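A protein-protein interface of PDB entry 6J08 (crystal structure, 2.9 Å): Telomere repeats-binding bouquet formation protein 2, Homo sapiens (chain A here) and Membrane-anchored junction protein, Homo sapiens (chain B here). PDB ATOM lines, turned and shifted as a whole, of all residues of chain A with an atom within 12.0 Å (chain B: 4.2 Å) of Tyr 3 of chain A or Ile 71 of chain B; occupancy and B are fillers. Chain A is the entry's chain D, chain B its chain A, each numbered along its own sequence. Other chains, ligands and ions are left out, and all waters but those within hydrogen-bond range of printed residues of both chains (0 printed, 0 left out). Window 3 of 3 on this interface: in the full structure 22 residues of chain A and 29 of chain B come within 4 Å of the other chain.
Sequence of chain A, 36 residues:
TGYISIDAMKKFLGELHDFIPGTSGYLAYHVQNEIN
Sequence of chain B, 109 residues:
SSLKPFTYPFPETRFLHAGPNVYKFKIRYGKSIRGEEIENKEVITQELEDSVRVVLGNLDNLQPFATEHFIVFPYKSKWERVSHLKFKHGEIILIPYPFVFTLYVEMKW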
ATOM      1  N   THR A   1     -12.796  19.798   1.515  1.00  0.00           N
ATOM      2  CA  THR A   1     -13.156  21.010   0.718  1.00  0.00           C
ATOM      3  C   THR A   1     -12.115  21.251  -0.381  1.00  0.00           C
ATOM      4  O   THR A   1     -10.908  21.149  -0.094  1.00  0.00           O
ATOM      5  CB  THR A   1     -13.308  22.260   1.592  1.00  0.00           C
ATOM      6  OG1 THR A   1     -14.509  22.075   2.345  1.00  0.00           O
ATOM      7  CG2 THR A   1     -13.385  23.541   0.786  1.00  0.00           C
ATOM      8  N   GLY A   2     -12.602  21.647  -1.561  1.00  0.00           N
ATOM      9  CA  GLY A   2     -11.915  21.568  -2.862  1.00  0.00           C
ATOM     10  C   GLY A   2     -12.696  20.654  -3.791  1.00  0.00           C
ATOM     11  O   GLY A   2     -13.273  19.668  -3.295  1.00  0.00           O
ATOM     12  N   TYR A   3     -12.754  20.988  -5.081  1.00  0.00           N
ATOM     13  CA  TYR A   3     -13.386  20.158  -6.139  1.00  0.00           C
ATOM     14  C   TYR A   3     -12.301  19.340  -6.830  1.00  0.00           C
ATOM     15  O   TYR A   3     -11.150  19.778  -6.831  1.00  0.00           O
ATOM     16  CB  TYR A   3     -14.150  21.039  -7.123  1.00  0.00           C
ATOM     17  CG  TYR A   3     -15.320  21.741  -6.487  1.00  0.00           C
ATOM     18  CD1 TYR A   3     -15.298  23.104  -6.225  1.00  0.00           C
ATOM     19  CD2 TYR A   3     -16.434  21.025  -6.100  1.00  0.00           C
ATOM     20  CE1 TYR A   3     -16.380  23.738  -5.638  1.00  0.00           C
ATOM     21  CE2 TYR A   3     -17.518  21.642  -5.502  1.00  0.00           C
ATOM     22  CZ  TYR A   3     -17.492  23.001  -5.265  1.00  0.00           C
ATOM     23  OH  TYR A   3     -18.565  23.606  -4.681  1.00  0.00           O
ATOM     24  N   ILE A   4     -12.659  18.177  -7.367  1.00  0.00           N
ATOM     25  CA  ILE A   4     -11.734  17.307  -8.142  1.00  0.00           C
ATOM     26  C   ILE A   4     -11.278  18.098  -9.369  1.00  0.00           C
ATOM     27  O   ILE A   4     -12.114  18.795  -9.991  1.00  0.00           O
ATOM     28  CB  ILE A   4     -12.421  15.979  -8.530  1.00  0.00           C
ATOM     29  CG1 ILE A   4     -11.410  14.916  -8.965  1.00  0.00           C
ATOM     30  CG2 ILE A   4     -13.484  16.207  -9.603  1.00  0.00           C
ATOM     31  CD1 ILE A   4     -11.961  13.511  -8.960  1.00  0.00           C
ATOM     32  N   SER A   5      -9.996  17.996  -9.705  1.00  0.00           N
ATOM     33  CA  SER A   5      -9.413  18.548 -10.952  1.00  0.00           C
ATOM     34  C   SER A   5      -9.940  17.772 -12.155  1.00  0.00           C
ATOM     35  O   SER A   5      -9.967  16.528 -12.106  1.00  0.00           O
ATOM     36  CB  SER A   5      -7.930  18.484 -10.947  1.00  0.00           C
ATOM     37  OG  SER A   5      -7.444  18.824 -12.230  1.00  0.00           O
ATOM     38  N   ILE A   6     -10.302  18.494 -13.208  1.00  0.00           N
ATOM     39  CA  ILE A   6     -10.597  17.906 -14.541  1.00  0.00           C
ATOM     40  C   ILE A   6      -9.479  16.923 -14.931  1.00  0.00           C
ATOM     41  O   ILE A   6      -9.798  15.898 -15.541  1.00  0.00           O
ATOM     42  CB  ILE A   6     -10.794  19.017 -15.588  1.00  0.00           C
ATOM     43  CG1 ILE A   6     -11.396  18.463 -16.876  1.00  0.00           C
ATOM     44  CG2 ILE A   6      -9.500  19.748 -15.850  1.00  0.00           C
ATOM     45  CD1 ILE A   6     -11.935  19.525 -17.786  1.00  0.00           C
ATOM     46  N   ASP A   7      -8.218  17.207 -14.590  1.00  0.00           N
ATOM     47  CA  ASP A   7      -7.065  16.336 -14.948  1.00  0.00           C
ATOM     48  C   ASP A   7      -7.283  14.908 -14.429  1.00  0.00           C
ATOM     49  O   ASP A   7      -6.747  13.985 -15.069  1.00  0.00           O
ATOM     50  CB  ASP A   7      -5.739  16.885 -14.419  1.00  0.00           C
ATOM     51  CG  ASP A   7      -5.213  18.097 -15.170  1.00  0.00           C
ATOM     52  OD1 ASP A   7      -5.717  18.382 -16.278  1.00  0.00           O
ATOM     53  OD2 ASP A   7      -4.287  18.741 -14.640  1.00  0.00           O
ATOM     54  N   ALA A   8      -8.015  14.727 -13.323  1.00  0.00           N
ATOM     55  CA  ALA A   8      -8.238  13.420 -12.653  1.00  0.00           C
ATOM     56  C   ALA A   8      -9.564  12.798 -13.114  1.00  0.00           C
ATOM     57  O   ALA A   8      -9.789  11.603 -12.876  1.00  0.00           O
ATOM     58  CB  ALA A   8      -8.207  13.606 -11.153  1.00  0.00           C
ATOM     59  N   MET A   9     -10.433  13.602 -13.715  1.00  0.00           N
ATOM     60  CA  MET A   9     -11.680  13.144 -14.377  1.00  0.00           C
ATOM     61  C   MET A   9     -11.316  12.429 -15.692  1.00  0.00           C
ATOM     62  O   MET A   9     -10.584  13.003 -16.530  1.00  0.00           O
ATOM     63  CB  MET A   9     -12.592  14.351 -14.636  1.00  0.00           C
ATOM     64  CG  MET A   9     -13.046  15.046 -13.364  1.00  0.00           C
ATOM     65  SD  MET A   9     -13.996  13.884 -12.354  1.00  0.00           S
ATOM     66  CE  MET A   9     -15.555  13.932 -13.229  1.00  0.00           C
ATOM     67  N   PRO B  64     -19.243  17.875  -9.293  1.00  0.00           N
ATOM     68  CA  PRO B  64     -18.614  19.134  -9.679  1.00  0.00           C
ATOM     69  C   PRO B  64     -17.115  18.905  -9.902  1.00  0.00           C
ATOM     70  O   PRO B  64     -16.528  18.093  -9.164  1.00  0.00           O
ATOM     71  CB  PRO B  64     -18.869  20.066  -8.493  1.00  0.00           C
ATOM     72  CG  PRO B  64     -20.011  19.423  -7.760  1.00  0.00           C
ATOM     73  CD  PRO B  64     -19.848  17.934  -7.962  1.00  0.00           C
ATOM     74  N   PHE B  65     -16.530  19.604 -10.879  1.00  0.00           N
ATOM     75  CA  PHE B  65     -15.063  19.569 -11.122  1.00  0.00           C
ATOM     76  C   PHE B  65     -14.503  20.983 -11.369  1.00  0.00           C
ATOM     77  O   PHE B  65     -15.249  21.949 -11.684  1.00  0.00           O
ATOM     78  CB  PHE B  65     -14.730  18.585 -12.251  1.00  0.00           C
ATOM     79  CG  PHE B  65     -15.405  18.852 -13.573  1.00  0.00           C
ATOM     80  CD1 PHE B  65     -16.619  18.268 -13.884  1.00  0.00           C
ATOM     81  CD2 PHE B  65     -14.815  19.679 -14.513  1.00  0.00           C
ATOM     82  CE1 PHE B  65     -17.241  18.528 -15.098  1.00  0.00           C
ATOM     83  CE2 PHE B  65     -15.435  19.939 -15.731  1.00  0.00           C
ATOM     84  CZ  PHE B  65     -16.654  19.367 -16.019  1.00  0.00           C
ATOM     85  N   PHE B  70     -12.449  27.492 -14.274  1.00  0.00           N
ATOM     86  CA  PHE B  70     -13.877  27.321 -13.872  1.00  0.00           C
ATOM     87  C   PHE B  70     -14.086  26.220 -12.842  1.00  0.00           C
ATOM     88  O   PHE B  70     -13.207  25.355 -12.661  1.00  0.00           O
ATOM     89  CB  PHE B  70     -14.776  26.985 -15.060  1.00  0.00           C
ATOM     90  CG  PHE B  70     -14.658  27.962 -16.198  1.00  0.00           C
ATOM     91  CD1 PHE B  70     -14.277  27.536 -17.459  1.00  0.00           C
ATOM     92  CD2 PHE B  70     -14.892  29.314 -15.986  1.00  0.00           C
ATOM     93  CE1 PHE B  70     -14.182  28.441 -18.500  1.00  0.00           C
ATOM     94  CE2 PHE B  70     -14.782  30.216 -17.027  1.00  0.00           C
ATOM     95  CZ  PHE B  70     -14.430  29.778 -18.279  1.00  0.00           C
ATOM     96  N   ILE B  71     -15.249  26.298 -12.189  1.00  0.00           N
ATOM     97  CA  ILE B  71     -15.908  25.149 -11.508  1.00  0.00           C
ATOM     98  C   ILE B  71     -17.173  24.765 -12.289  1.00  0.00           C
ATOM     99  O   ILE B  71     -18.116  25.564 -12.354  1.00  0.00           O
ATOM    100  CB  ILE B  71     -16.188  25.485 -10.040  1.00  0.00           C
ATOM    101  CG1 ILE B  71     -14.876  25.777  -9.313  1.00  0.00           C
ATOM    102  CG2 ILE B  71     -16.961  24.353  -9.371  1.00  0.00           C
ATOM    103  CD1 ILE B  71     -15.061  26.404  -7.957  1.00  0.00           C
ATOM    104  N   VAL B  72     -17.194  23.566 -12.863  1.00  0.00           N
ATOM    105  CA  VAL B  72     -18.381  23.039 -13.598  1.00  0.00           C
ATOM    106  C   VAL B  72     -19.180  22.098 -12.685  1.00  0.00           C
ATOM    107  O   VAL B  72     -18.600  21.112 -12.156  1.00  0.00           O
ATOM    108  CB  VAL B  72     -17.926  22.383 -14.907  1.00  0.00           C
ATOM    109  CG1 VAL B  72     -19.083  21.910 -15.753  1.00  0.00           C
ATOM    110  CG2 VAL B  72     -17.073  23.369 -15.682  1.00  0.00           C
ATOM    111  N   PHE B  73     -20.436  22.471 -12.451  1.00  0.00           N
ATOM    112  CA  PHE B  73     -21.482  21.664 -11.788  1.00  0.00           C
ATOM    113  C   PHE B  73     -22.406  21.117 -12.876  1.00  0.00           C
ATOM    114  O   PHE B  73     -23.360  21.798 -13.284  1.00  0.00           O
ATOM    115  CB  PHE B  73     -22.254  22.523 -10.785  1.00  0.00           C
ATOM    116  CG  PHE B  73     -21.416  23.226  -9.750  1.00  0.00           C
ATOM    117  CD1 PHE B  73     -20.858  24.475 -10.019  1.00  0.00           C
ATOM    118  CD2 PHE B  73     -21.222  22.661  -8.494  1.00  0.00           C
ATOM    119  CE1 PHE B  73     -20.104  25.133  -9.062  1.00  0.00           C
ATOM    120  CE2 PHE B  73     -20.453  23.321  -7.546  1.00  0.00           C
ATOM    121  CZ  PHE B  73     -19.895  24.547  -7.833  1.00  0.00           C
ATOM    122  N   TYR B 104     -23.624  24.134 -15.244  1.00  0.00           N
ATOM    123  CA  TYR B 104     -23.565  25.450 -14.568  1.00  0.00           C
ATOM    124  C   TYR B 104     -22.095  25.750 -14.314  1.00  0.00           C
ATOM    125  O   TYR B 104     -21.505  25.103 -13.446  1.00  0.00           O
ATOM    126  CB  TYR B 104     -24.351  25.454 -13.259  1.00  0.00           C
ATOM    127  CG  TYR B 104     -25.824  25.159 -13.369  1.00  0.00           C
ATOM    128  CD1 TYR B 104     -26.287  23.847 -13.297  1.00  0.00           C
ATOM    129  CD2 TYR B 104     -26.762  26.168 -13.502  1.00  0.00           C
ATOM    130  CE1 TYR B 104     -27.638  23.544 -13.346  1.00  0.00           C
ATOM    131  CE2 TYR B 104     -28.118  25.882 -13.556  1.00  0.00           C
ATOM    132  CZ  TYR B 104     -28.556  24.567 -13.471  1.00  0.00           C
ATOM    133  OH  TYR B 104     -29.871  24.232 -13.512  1.00  0.00           O
ATOM    134  N   VAL B 105     -21.554  26.708 -15.064  1.00  0.00           N
ATOM    135  CA  VAL B 105     -20.122  27.124 -15.078  1.00  0.00           C
ATOM    136  C   VAL B 105     -19.948  28.395 -14.237  1.00  0.00           C
ATOM    137  O   VAL B 105     -20.479  29.437 -14.650  1.00  0.00           O
ATOM    138  CB  VAL B 105     -19.705  27.369 -16.538  1.00  0.00           C
ATOM    139  CG1 VAL B 105     -18.265  27.842 -16.653  1.00  0.00           C
ATOM    140  CG2 VAL B 105     -19.966  26.143 -17.407  1.00  0.00           C
ATOM    141  N   GLU B 106     -19.215  28.312 -13.126  1.00  0.00           N
ATOM    142  CA  GLU B 106     -18.792  29.469 -12.293  1.00  0.00           C
ATOM    143  C   GLU B 106     -17.273  29.689 -12.439  1.00  0.00           C
ATOM    144  O   GLU B 106     -16.574  28.717 -12.833  1.00  0.00           O
ATOM    145  CB  GLU B 106     -19.212  29.197 -10.848  1.00  0.00           C
ATOM    146  CG  GLU B 106     -20.713  29.026 -10.659  1.00  0.00           C
ATOM    147  CD  GLU B 106     -21.549  30.273 -10.890  1.00  0.00           C
ATOM    148  OE1 GLU B 106     -21.057  31.205 -11.548  1.00  0.00           O
ATOM    149  OE2 GLU B 106     -22.680  30.317 -10.406  1.00  0.00           O
ATOM    150  N   LYS B 108     -13.601  30.110 -10.620  1.00  0.00           N
ATOM    151  CA  LYS B 108     -13.072  29.609  -9.315  1.00  0.00           C
ATOM    152  C   LYS B 108     -12.943  30.749  -8.271  1.00  0.00           C
ATOM    153  O   LYS B 108     -13.390  30.536  -7.111  1.00  0.00           O
ATOM    154  CB  LYS B 108     -11.717  28.930  -9.497  1.00  0.00           C
ATOM    155  CG  LYS B 108     -11.717  27.726 -10.406  1.00  0.00           C
ATOM    156  CD  LYS B 108     -10.342  27.376 -10.890  1.00  0.00           C
ATOM    157  CE  LYS B 108      -9.514  26.714  -9.819  1.00  0.00           C
ATOM    158  NZ  LYS B 108      -8.153  26.430 -10.325  1.00  0.00           N
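The backbone carbonyl oxygen (O) of Phe 65 of chain B is in hydrogen-bond range of the backbone NH (N) of Val 72 of chain B (2.8 Å).
The backbone carbonyl oxygen (O) of Glu 106 of chain B sits at hydrogen-bond distance from the backbone NH (N) of Ile 71 of chain B, at 2.8 Å.
O of Tyr 104 of chain B is in hydrogen-bond range of N of Phe 73 of chain B (3.0 Å).
Of the 9 printed residues of chain A, 2 touch a printed residue of chain B.
Hydrophobic or aromatic side chains of chain A within 4 Å of the printed part of chain B: Tyr 3 and Ile 4.
Among the printed residues, merely in contact across the chains: Tyr 3 of chain A with Pro 64 of chain B (3.5 Å), Tyr 3 of chain A with Ile 71 of chain B (3.7 Å), Tyr 3 of chain A with Phe 73 of chain B (3.4 Å), Ile 4 of chain A with Pro 64 of chain B (3.6 Å) and Ile 4 of chain A with Phe 65 of chain B (3.3 Å).
Of chain B, only Pro 64, Ile 71 and Phe 73 come within 4 Å of Tyr 3 of chain A.
Ile 71 of chain B touches just one residue of chain A: Tyr 3.
Printed residues of chain A within 4 Å of Pro 64 of chain B: Tyr 3 and Ile 4.
Phe 65 of chain B touches one residue of chain A.
No residue of chain A comes within 4 Å of Phe 70 of chain B.
No residue of chain A comes within 4 Å of Lys 108 of chain B.
Of the printed residues of chain B, Ile 4 of chain A touches Pro 64 and Phe 65.
Ala 8 of chain A touches none of the printed residues of chain B.
Asp 7 of chain A touches none of the printed residues of chain B.
The nearest printed residue of chain B that does not touch Ile 4 of chain A is Phe 70 of chain B (7.2 Å).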
